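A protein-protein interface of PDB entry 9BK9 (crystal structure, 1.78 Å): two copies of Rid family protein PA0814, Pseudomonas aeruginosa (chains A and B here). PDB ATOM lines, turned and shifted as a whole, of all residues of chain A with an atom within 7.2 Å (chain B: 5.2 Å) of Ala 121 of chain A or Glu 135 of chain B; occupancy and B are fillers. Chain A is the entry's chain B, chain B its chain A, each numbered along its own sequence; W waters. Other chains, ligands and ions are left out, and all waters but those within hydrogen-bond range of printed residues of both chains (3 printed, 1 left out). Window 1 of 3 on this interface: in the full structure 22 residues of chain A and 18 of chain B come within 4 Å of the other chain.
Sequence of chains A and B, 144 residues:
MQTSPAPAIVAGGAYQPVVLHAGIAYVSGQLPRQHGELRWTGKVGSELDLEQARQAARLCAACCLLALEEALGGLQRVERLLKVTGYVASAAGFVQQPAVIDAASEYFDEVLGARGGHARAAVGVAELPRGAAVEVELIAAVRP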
ATOM      1  N   LYS A  83     -17.951  38.554  -6.693  1.00  0.00           N
ATOM      2  CA  LYS A  83     -18.126  37.358  -7.500  1.00  0.00           C
ATOM      3  C   LYS A  83     -17.363  36.231  -6.836  1.00  0.00           C
ATOM      4  O   LYS A  83     -16.237  36.425  -6.372  1.00  0.00           O
ATOM      5  CB  LYS A  83     -17.652  37.582  -8.958  1.00  0.00           C
ATOM      6  CG  LYS A  83     -17.720  36.353  -9.849  1.00  0.00           C
ATOM      7  CD  LYS A  83     -19.179  36.023  -9.981  1.00  0.00           C
ATOM      8  CE  LYS A  83     -19.646  35.005 -11.058  1.00  0.00           C
ATOM      9  NZ  LYS A  83     -19.271  35.345 -12.468  1.00  0.00           N
ATOM     10  N   VAL A  84     -17.976  35.059  -6.782  1.00  0.00           N
ATOM     11  CA  VAL A  84     -17.346  33.875  -6.207  1.00  0.00           C
ATOM     12  C   VAL A  84     -17.272  32.824  -7.304  1.00  0.00           C
ATOM     13  O   VAL A  84     -18.241  32.641  -8.046  1.00  0.00           O
ATOM     14  CB  VAL A  84     -18.136  33.342  -4.998  1.00  0.00           C
ATOM     15  CG1 VAL A  84     -17.585  31.999  -4.544  1.00  0.00           C
ATOM     16  CG2 VAL A  84     -18.136  34.357  -3.847  1.00  0.00           C
ATOM     17  N   THR A  85     -16.132  32.144  -7.429  1.00  0.00           N
ATOM     18  CA  THR A  85     -16.045  31.000  -8.331  1.00  0.00           C
ATOM     19  C   THR A  85     -15.724  29.760  -7.523  1.00  0.00           C
ATOM     20  O   THR A  85     -14.745  29.743  -6.765  1.00  0.00           O
ATOM     21  CB  THR A  85     -14.998  31.188  -9.436  1.00  0.00           C
ATOM     22  OG1 THR A  85     -15.279  32.388 -10.172  1.00  0.00           O
ATOM     23  CG2 THR A  85     -15.039  30.011 -10.402  1.00  0.00           C
ATOM     24  N   GLY A  86     -16.560  28.733  -7.671  1.00  0.00           N
ATOM     25  CA  GLY A  86     -16.344  27.496  -6.953  1.00  0.00           C
ATOM     26  C   GLY A  86     -16.037  26.343  -7.888  1.00  0.00           C
ATOM     27  O   GLY A  86     -16.839  26.022  -8.772  1.00  0.00           O
ATOM     28  N   TYR A  87     -14.902  25.688  -7.681  1.00  0.00           N
ATOM     29  CA  TYR A  87     -14.516  24.524  -8.457  1.00  0.00           C
ATOM     30  C   TYR A  87     -14.684  23.301  -7.563  1.00  0.00           C
ATOM     31  O   TYR A  87     -14.191  23.284  -6.431  1.00  0.00           O
ATOM     32  CB  TYR A  87     -13.061  24.627  -8.936  1.00  0.00           C
ATOM     33  CG  TYR A  87     -12.710  25.930  -9.645  1.00  0.00           C
ATOM     34  CD1 TYR A  87     -12.978  26.099 -10.999  1.00  0.00           C
ATOM     35  CD2 TYR A  87     -12.073  26.960  -8.969  1.00  0.00           C
ATOM     36  CE1 TYR A  87     -12.643  27.285 -11.665  1.00  0.00           C
ATOM     37  CE2 TYR A  87     -11.735  28.144  -9.623  1.00  0.00           C
ATOM     38  CZ  TYR A  87     -12.021  28.291 -10.972  1.00  0.00           C
ATOM     39  OH  TYR A  87     -11.692  29.465 -11.620  1.00  0.00           O
ATOM     40  N   GLN A  97     -22.925  20.320  -8.145  1.00  0.00           N
ATOM     41  CA  GLN A  97     -22.015  21.393  -7.740  1.00  0.00           C
ATOM     42  C   GLN A  97     -22.715  22.607  -7.133  1.00  0.00           C
ATOM     43  O   GLN A  97     -22.137  23.207  -6.206  1.00  0.00           O
ATOM     44  CB  GLN A  97     -21.148  21.842  -8.930  1.00  0.00           C
ATOM     45  CG  GLN A  97     -20.212  20.786  -9.480  1.00  0.00           C
ATOM     46  CD  GLN A  97     -20.917  19.835 -10.431  1.00  0.00           C
ATOM     47  OE1 GLN A  97     -22.064  20.075 -10.828  1.00  0.00           O
ATOM     48  NE2 GLN A  97     -20.239  18.741 -10.801  1.00  0.00           N
ATOM     49  N   PRO A  98     -23.899  23.058  -7.609  1.00  0.00           N
ATOM     50  CA  PRO A  98     -24.542  24.196  -6.930  1.00  0.00           C
ATOM     51  C   PRO A  98     -24.829  23.918  -5.473  1.00  0.00           C
ATOM     52  O   PRO A  98     -24.645  24.809  -4.644  1.00  0.00           O
ATOM     53  CB  PRO A  98     -25.834  24.409  -7.730  1.00  0.00           C
ATOM     54  CG  PRO A  98     -25.523  23.880  -9.077  1.00  0.00           C
ATOM     55  CD  PRO A  98     -24.640  22.681  -8.828  1.00  0.00           C
ATOM     56  N   ILE A 101     -21.444  24.361  -3.604  1.00  0.00           N
ATOM     57  CA  ILE A 101     -20.975  25.734  -3.456  1.00  0.00           C
ATOM     58  C   ILE A 101     -21.969  26.583  -2.664  1.00  0.00           C
ATOM     59  O   ILE A 101     -21.584  27.619  -2.085  1.00  0.00           O
ATOM     60  CB  ILE A 101     -20.659  26.310  -4.852  1.00  0.00           C
ATOM     61  CG1 ILE A 101     -19.604  25.438  -5.521  1.00  0.00           C
ATOM     62  CG2 ILE A 101     -20.155  27.753  -4.766  1.00  0.00           C
ATOM     63  CD1 ILE A 101     -18.328  25.266  -4.659  1.00  0.00           C
ATOM     64  N   HIS A 118     -23.402  37.985  -3.773  1.00  0.00           N
ATOM     65  CA  HIS A 118     -22.392  37.834  -4.812  1.00  0.00           C
ATOM     66  C   HIS A 118     -22.979  37.163  -6.040  1.00  0.00           C
ATOM     67  O   HIS A 118     -23.913  36.362  -5.947  1.00  0.00           O
ATOM     68  CB  HIS A 118     -21.215  37.007  -4.306  1.00  0.00           C
ATOM     69  CG  HIS A 118     -21.637  35.707  -3.697  1.00  0.00           C
ATOM     70  ND1 HIS A 118     -22.041  35.610  -2.382  1.00  0.00           N
ATOM     71  CD2 HIS A 118     -21.729  34.457  -4.213  1.00  0.00           C
ATOM     72  CE1 HIS A 118     -22.362  34.355  -2.115  1.00  0.00           C
ATOM     73  NE2 HIS A 118     -22.189  33.636  -3.210  1.00  0.00           N
ATOM     74  N   ALA A 119     -22.398  37.484  -7.191  1.00  0.00           N
ATOM     75  CA  ALA A 119     -22.577  36.625  -8.348  1.00  0.00           C
ATOM     76  C   ALA A 119     -21.717  35.375  -8.172  1.00  0.00           C
ATOM     77  O   ALA A 119     -20.803  35.339  -7.343  1.00  0.00           O
ATOM     78  CB  ALA A 119     -22.222  37.367  -9.637  1.00  0.00           C
ATOM     79  N   ARG A 120     -22.008  34.337  -8.955  1.00  0.00           N
ATOM     80  CA  ARG A 120     -21.365  33.054  -8.693  1.00  0.00           C
ATOM     81  C   ARG A 120     -21.250  32.215  -9.960  1.00  0.00           C
ATOM     82  O   ARG A 120     -22.082  32.304 -10.862  1.00  0.00           O
ATOM     83  CB  ARG A 120     -22.147  32.251  -7.648  1.00  0.00           C
ATOM     84  CG  ARG A 120     -21.319  31.213  -6.898  1.00  0.00           C
ATOM     85  CD  ARG A 120     -22.179  30.504  -5.858  1.00  0.00           C
ATOM     86  NE  ARG A 120     -23.056  29.517  -6.473  1.00  0.00           N
ATOM     87  CZ  ARG A 120     -23.957  28.814  -5.801  1.00  0.00           C
ATOM     88  NH1 ARG A 120     -24.155  29.006  -4.508  1.00  0.00           N
ATOM     89  NH2 ARG A 120     -24.668  27.887  -6.440  1.00  0.00           N
ATOM     90  N   ALA A 121     -20.210  31.384 -10.007  1.00  0.00           N
ATOM     91  CA  ALA A 121     -20.131  30.279 -10.953  1.00  0.00           C
ATOM     92  C   ALA A 121     -19.715  29.036 -10.183  1.00  0.00           C
ATOM     93  O   ALA A 121     -18.957  29.120  -9.213  1.00  0.00           O
ATOM     94  CB  ALA A 121     -19.140  30.555 -12.097  1.00  0.00           C
ATOM     95  N   ALA A 122     -20.228  27.884 -10.610  1.00  0.00           N
ATOM     96  CA  ALA A 122     -19.940  26.607  -9.962  1.00  0.00           C
ATOM     97  C   ALA A 122     -19.697  25.579 -11.053  1.00  0.00           C
ATOM     98  O   ALA A 122     -20.568  25.350 -11.899  1.00  0.00           O
ATOM     99  CB  ALA A 122     -21.093  26.160  -9.061  1.00  0.00           C
ATOM    100  N   VAL A 123     -18.523  24.966 -11.057  1.00  0.00           N
ATOM    101  CA  VAL A 123     -18.183  24.049 -12.138  1.00  0.00           C
ATOM    102  C   VAL A 123     -17.545  22.797 -11.558  1.00  0.00           C
ATOM    103  O   VAL A 123     -16.922  22.832 -10.493  1.00  0.00           O
ATOM    104  CB  VAL A 123     -17.254  24.710 -13.176  1.00  0.00           C
ATOM    105  CG1 VAL A 123     -17.934  25.922 -13.838  1.00  0.00           C
ATOM    106  CG2 VAL A 123     -15.955  25.137 -12.523  1.00  0.00           C
ATOM    107  N   GLY A 124     -17.704  21.688 -12.270  1.00  0.00           N
ATOM    108  CA  GLY A 124     -17.098  20.437 -11.863  1.00  0.00           C
ATOM    109  C   GLY A 124     -15.804  20.178 -12.602  1.00  0.00           C
ATOM    110  O   GLY A 124     -15.811  19.966 -13.816  1.00  0.00           O
ATOM    111  N   GLY B  29     -22.693  32.499 -13.737  1.00  0.00           N
ATOM    112  CA  GLY B  29     -22.759  31.422 -14.705  1.00  0.00           C
ATOM    113  C   GLY B  29     -24.175  31.017 -15.054  1.00  0.00           C
ATOM    114  O   GLY B  29     -25.012  30.813 -14.165  1.00  0.00           O
ATOM    115  N   GLN B  30     -24.459  30.938 -16.349  1.00  0.00           N
ATOM    116  CA  GLN B  30     -25.775  30.576 -16.866  1.00  0.00           C
ATOM    117  C   GLN B  30     -25.690  29.227 -17.563  1.00  0.00           C
ATOM    118  O   GLN B  30     -24.714  28.946 -18.267  1.00  0.00           O
ATOM    119  CB  GLN B  30     -26.280  31.634 -17.856  1.00  0.00           C
ATOM    120  CG  GLN B  30     -26.328  33.052 -17.287  1.00  0.00           C
ATOM    121  CD  GLN B  30     -27.286  33.199 -16.124  1.00  0.00           C
ATOM    122  OE1 GLN B  30     -28.408  32.692 -16.164  1.00  0.00           O
ATOM    123  NE2 GLN B  30     -26.849  33.902 -15.076  1.00  0.00           N
ATOM    124  N   LEU B  31     -26.709  28.404 -17.363  1.00  0.00           N
ATOM    125  CA  LEU B  31     -26.849  27.110 -18.005  1.00  0.00           C
ATOM    126  C   LEU B  31     -27.701  27.244 -19.262  1.00  0.00           C
ATOM    127  O   LEU B  31     -28.340  28.274 -19.487  1.00  0.00           O
ATOM    128  CB  LEU B  31     -27.469  26.126 -17.016  1.00  0.00           C
ATOM    129  CG  LEU B  31     -26.732  25.944 -15.673  1.00  0.00           C
ATOM    130  CD1 LEU B  31     -27.413  24.826 -14.863  1.00  0.00           C
ATOM    131  CD2 LEU B  31     -25.253  25.616 -15.892  1.00  0.00           C
ATOM    132  N   CYS B  60     -26.966  29.789 -23.435  1.00  0.00           N
ATOM    133  CA  CYS B  60     -26.284  30.355 -22.267  1.00  0.00           C
ATOM    134  C   CYS B  60     -26.033  31.845 -22.446  1.00  0.00           C
ATOM    135  O   CYS B  60     -26.229  32.644 -21.517  1.00  0.00           O
ATOM    136  CB  CYS B  60     -24.944  29.648 -22.024  1.00  0.00           C
ATOM    137  SG  CYS B  60     -24.982  27.922 -21.581  1.00  0.00           S
ATOM    138  N   THR B  85     -16.284  33.849 -19.919  1.00  0.00           N
ATOM    139  CA  THR B  85     -15.693  32.551 -19.632  1.00  0.00           C
ATOM    140  C   THR B  85     -16.702  31.472 -19.987  1.00  0.00           C
ATOM    141  O   THR B  85     -17.854  31.518 -19.533  1.00  0.00           O
ATOM    142  CB  THR B  85     -15.269  32.411 -18.168  1.00  0.00           C
ATOM    143  OG1 THR B  85     -14.400  33.494 -17.819  1.00  0.00           O
ATOM    144  CG2 THR B  85     -14.502  31.120 -17.986  1.00  0.00           C
ATOM    145  N   GLY B  86     -16.272  30.533 -20.826  1.00  0.00           N
ATOM    146  CA  GLY B  86     -17.125  29.436 -21.252  1.00  0.00           C
ATOM    147  C   GLY B  86     -16.587  28.105 -20.780  1.00  0.00           C
ATOM    148  O   GLY B  86     -15.433  27.767 -21.052  1.00  0.00           O
ATOM    149  N   TYR B  87     -17.417  27.342 -20.073  1.00  0.00           N
ATOM    150  CA  TYR B  87     -17.079  26.013 -19.586  1.00  0.00           C
ATOM    151  C   TYR B  87     -17.876  24.997 -20.389  1.00  0.00           C
ATOM    152  O   TYR B  87     -19.092  25.147 -20.550  1.00  0.00           O
ATOM    153  CB  TYR B  87     -17.426  25.870 -18.101  1.00  0.00           C
ATOM    154  CG  TYR B  87     -16.826  26.947 -17.230  1.00  0.00           C
ATOM    155  CD1 TYR B  87     -15.532  26.824 -16.746  1.00  0.00           C
ATOM    156  CD2 TYR B  87     -17.560  28.059 -16.857  1.00  0.00           C
ATOM    157  CE1 TYR B  87     -14.977  27.788 -15.937  1.00  0.00           C
ATOM    158  CE2 TYR B  87     -17.009  29.031 -16.038  1.00  0.00           C
ATOM    159  CZ  TYR B  87     -15.720  28.882 -15.584  1.00  0.00           C
ATOM    160  OH  TYR B  87     -15.181  29.853 -14.769  1.00  0.00           O
ATOM    161  N   VAL B  88     -17.197  23.988 -20.909  1.00  0.00           N
ATOM    162  CA  VAL B  88     -17.843  22.978 -21.742  1.00  0.00           C
ATOM    163  C   VAL B  88     -17.621  21.626 -21.079  1.00  0.00           C
ATOM    164  O   VAL B  88     -16.473  21.210 -20.899  1.00  0.00           O
ATOM    165  CB  VAL B  88     -17.273  22.982 -23.167  1.00  0.00           C
ATOM    166  CG1 VAL B  88     -17.989  21.919 -24.005  1.00  0.00           C
ATOM    167  CG2 VAL B  88     -17.383  24.383 -23.804  1.00  0.00           C
ATOM    168  N   LEU B 128     -20.952  19.650 -15.211  1.00  0.00           N
ATOM    169  CA  LEU B 128     -21.594  20.924 -14.940  1.00  0.00           C
ATOM    170  C   LEU B 128     -22.894  20.722 -14.172  1.00  0.00           C
ATOM    171  O   LEU B 128     -23.442  19.612 -14.136  1.00  0.00           O
ATOM    172  CB  LEU B 128     -21.854  21.704 -16.241  1.00  0.00           C
ATOM    173  CG  LEU B 128     -20.603  22.338 -16.882  1.00  0.00           C
ATOM    174  CD1 LEU B 128     -21.022  22.966 -18.219  1.00  0.00           C
ATOM    175  CD2 LEU B 128     -19.907  23.382 -15.990  1.00  0.00           C
ATOM    176  N   PRO B 129     -23.385  21.772 -13.505  1.00  0.00           N
ATOM    177  CA  PRO B 129     -24.643  21.670 -12.748  1.00  0.00           C
ATOM    178  C   PRO B 129     -25.767  21.047 -13.559  1.00  0.00           C
ATOM    179  O   PRO B 129     -26.013  21.428 -14.707  1.00  0.00           O
ATOM    180  CB  PRO B 129     -24.950  23.129 -12.401  1.00  0.00           C
ATOM    181  CG  PRO B 129     -23.614  23.752 -12.267  1.00  0.00           C
ATOM    182  CD  PRO B 129     -22.752  23.090 -13.314  1.00  0.00           C
ATOM    183  N   ALA B 133     -24.570  20.976 -20.613  1.00  0.00           N
ATOM    184  CA  ALA B 133     -23.455  20.799 -21.543  1.00  0.00           C
ATOM    185  C   ALA B 133     -22.472  21.969 -21.512  1.00  0.00           C
ATOM    186  O   ALA B 133     -21.276  21.780 -21.785  1.00  0.00           O
ATOM    187  CB  ALA B 133     -23.986  20.585 -22.958  1.00  0.00           C
ATOM    188  N   VAL B 134     -22.963  23.176 -21.236  1.00  0.00           N
ATOM    189  CA  VAL B 134     -22.192  24.416 -21.331  1.00  0.00           C
ATOM    190  C   VAL B 134     -22.629  25.333 -20.197  1.00  0.00           C
ATOM    191  O   VAL B 134     -23.800  25.346 -19.805  1.00  0.00           O
ATOM    192  CB  VAL B 134     -22.390  25.123 -22.706  1.00  0.00           C
ATOM    193  CG1 VAL B 134     -21.552  26.409 -22.826  1.00  0.00           C
ATOM    194  CG2 VAL B 134     -22.055  24.186 -23.876  1.00  0.00           C
ATOM    195  N   GLU B 135     -21.688  26.126 -19.685  1.00  0.00           N
ATOM    196  CA  GLU B 135     -22.006  27.186 -18.732  1.00  0.00           C
ATOM    197  C   GLU B 135     -21.206  28.418 -19.124  1.00  0.00           C
ATOM    198  O   GLU B 135     -20.012  28.302 -19.423  1.00  0.00           O
ATOM    199  CB  GLU B 135     -21.689  26.761 -17.286  1.00  0.00           C
ATOM    200  CG  GLU B 135     -21.825  27.881 -16.259  1.00  0.00           C
ATOM    201  CD  GLU B 135     -21.597  27.428 -14.796  1.00  0.00           C
ATOM    202  OE1 GLU B 135     -21.557  26.207 -14.498  1.00  0.00           O
ATOM    203  OE2 GLU B 135     -21.407  28.306 -13.940  1.00  0.00           O
ATOM    204  N   VAL B 136     -21.845  29.588 -19.153  1.00  0.00           N
ATOM    205  CA  VAL B 136     -21.170  30.822 -19.575  1.00  0.00           C
ATOM    206  C   VAL B 136     -21.343  31.886 -18.502  1.00  0.00           C
ATOM    207  O   VAL B 136     -22.453  32.098 -17.998  1.00  0.00           O
ATOM    208  CB  VAL B 136     -21.691  31.329 -20.935  1.00  0.00           C
ATOM    209  CG1 VAL B 136     -21.006  32.652 -21.332  1.00  0.00           C
ATOM    210  CG2 VAL B 136     -21.463  30.260 -22.019  1.00  0.00           C
ATOM    211  N   GLU B 137     -20.251  32.552 -18.146  1.00  0.00           N
ATOM    212  CA  GLU B 137     -20.322  33.699 -17.247  1.00  0.00           C
ATOM    213  C   GLU B 137     -19.682  34.909 -17.914  1.00  0.00           C
ATOM    214  O   GLU B 137     -18.929  34.767 -18.886  1.00  0.00           O
ATOM    215  CB  GLU B 137     -19.646  33.377 -15.915  1.00  0.00           C
ATOM    216  CG  GLU B 137     -18.190  33.011 -16.047  1.00  0.00           C
ATOM    217  CD  GLU B 137     -17.527  32.795 -14.689  1.00  0.00           C
ATOM    218  OE1 GLU B 137     -18.011  33.372 -13.692  1.00  0.00           O
ATOM    219  OE2 GLU B 137     -16.516  32.068 -14.618  1.00  0.00           O
HETATM  220  O   HOH W   1     -12.453  30.018 -14.144  1.00  0.00           O
HETATM  221  O   HOH W   2     -23.111  27.947 -11.908  1.00  0.00           O
HETATM  222  O   HOH W   3     -24.726  30.471 -11.476  1.00  0.00           O
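N of Gly 29 of chain B is in hydrogen-bond range of O of Arg 120 of chain A (2.9 Å).
NZ of Lys 83 of chain A lies within salt-bridge range of OE1 of Glu 137 of chain B, at 2.6 Å.
The side-chain amide oxygen (OE1) of Gln 97 of chain A sits close to the backbone nitrogen (N) of Pro 129 of chain B.
The side-chain carboxylate (OE1) of Glu 135 of chain B sits close to the backbone carbonyl oxygen (O) of Ala 122 of chain A (2.9 Å).
OH of Tyr 87 of chain B is in hydrogen-bond range of OE2 of Glu 137 of chain B, 2.6 Å away.
O of Gly 86 of chain A sits at hydrogen-bond distance from N of Val 123 of chain A, at 3.0 Å.
The backbone carbonyl oxygen of Thr 85 of chain B sits at hydrogen-bond distance from the backbone NH of Glu 137 of chain B (3.0 Å).
The backbone carbonyl oxygen (O) of Val 84 of chain A is in hydrogen-bond range of the backbone NH (N) of Ala 121 of chain A, 3.1 Å away.
N of Tyr 87 of chain B lies within hydrogen-bond range of O of Glu 135 of chain B, at 2.8 Å.
The backbone NH (N) of Gly 86 of chain A is in hydrogen-bond range of the backbone carbonyl oxygen (O) of Ala 121 of chain A (2.9 Å).
Among the printed residues, merely in contact across the chains: Gln 97 of chain A with Leu 128 of chain B (3.5 Å), Pro 98 of chain A with Pro 129 of chain B (3.5 Å), Ala 121 of chain A with Glu 135 of chain B (3.7 Å), Ala 121 of chain A with Glu 137 of chain B (3.4 Å), Ala 122 of chain A with Pro 129 of chain B (3.4 Å), Val 123 of chain A with Tyr 87 of chain B (3.7 Å), Val 123 of chain A with Leu 128 of chain B (3.9 Å) and Val 123 of chain A with Glu 135 of chain B (3.7 Å).
Of the printed residues of chain B, Pro 98 of chain A touches Pro 129.
Ala 119 of chain A touches none of the printed residues of chain B.
Of the printed residues of chain B, Ala 121 of chain A touches Glu 135 and Glu 137.
Printed residues of chain B within 4 Å of Val 123 of chain A: Tyr 87 (3.7 Å), Leu 128 (3.9 Å) and Glu 135 (3.7 Å).
Of the printed residues of chain A, Tyr 87 of chain B touches Val 123 (3.7 Å).
Glu 135 of chain B touches three residues of chain A.
The nearest residue of chain B that does not touch Ala 121 of chain A is Gly 29 of chain B (4.4 Å).
The nearest residue of chain A that does not touch Glu 135 of chain B is Arg 120 of chain A (5.1 Å).
Of the 15 printed residues of chain B, 6 touch a printed residue of chain A.
Printed residues of chain B that touch a printed residue of chain A: Gly 29, Tyr 87, Leu 128, Pro 129, Glu 135 and Glu 137.
Of the 15 printed residues of chain A, 7 touch a printed residue of chain B.
Printed residues of chain A that touch a printed residue of chain B: Lys 83, Gln 97, Pro 98, Arg 120, Ala 121, Ala 122 and Val 123.
Hydrophobic or aromatic side chains of chain A that line the printed part of chain B: Pro 98, Ala 121 and Val 123.
Among the printed residues, Asp or Glu carboxylates within 4 Å of a Lys or Arg side-chain nitrogen of the other chain: Lys 83 of chain A with Glu 137 of chain B (2.6 Å).
3 positions are printed for both chains.
Of the 12 pairs that touch across the chains among the printed residues, none has its exchanged pair printed and touching as well.
Water W2 lies within hydrogen-bond range of the side-chain carboxylate of Glu 135 of chain B (2.7 Å) and the backbone NH of Ala 122 of chain A (3.2 Å).
Water W1 bridges OH of Tyr 87 of chain A (2.7 Å) and OH of Tyr 87 of chain B (2.8 Å).
Water W3 lies within hydrogen-bond range of O of Gly 29 of chain B (2.7 Å) and O of Arg 120 of chain A (3.3 Å).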
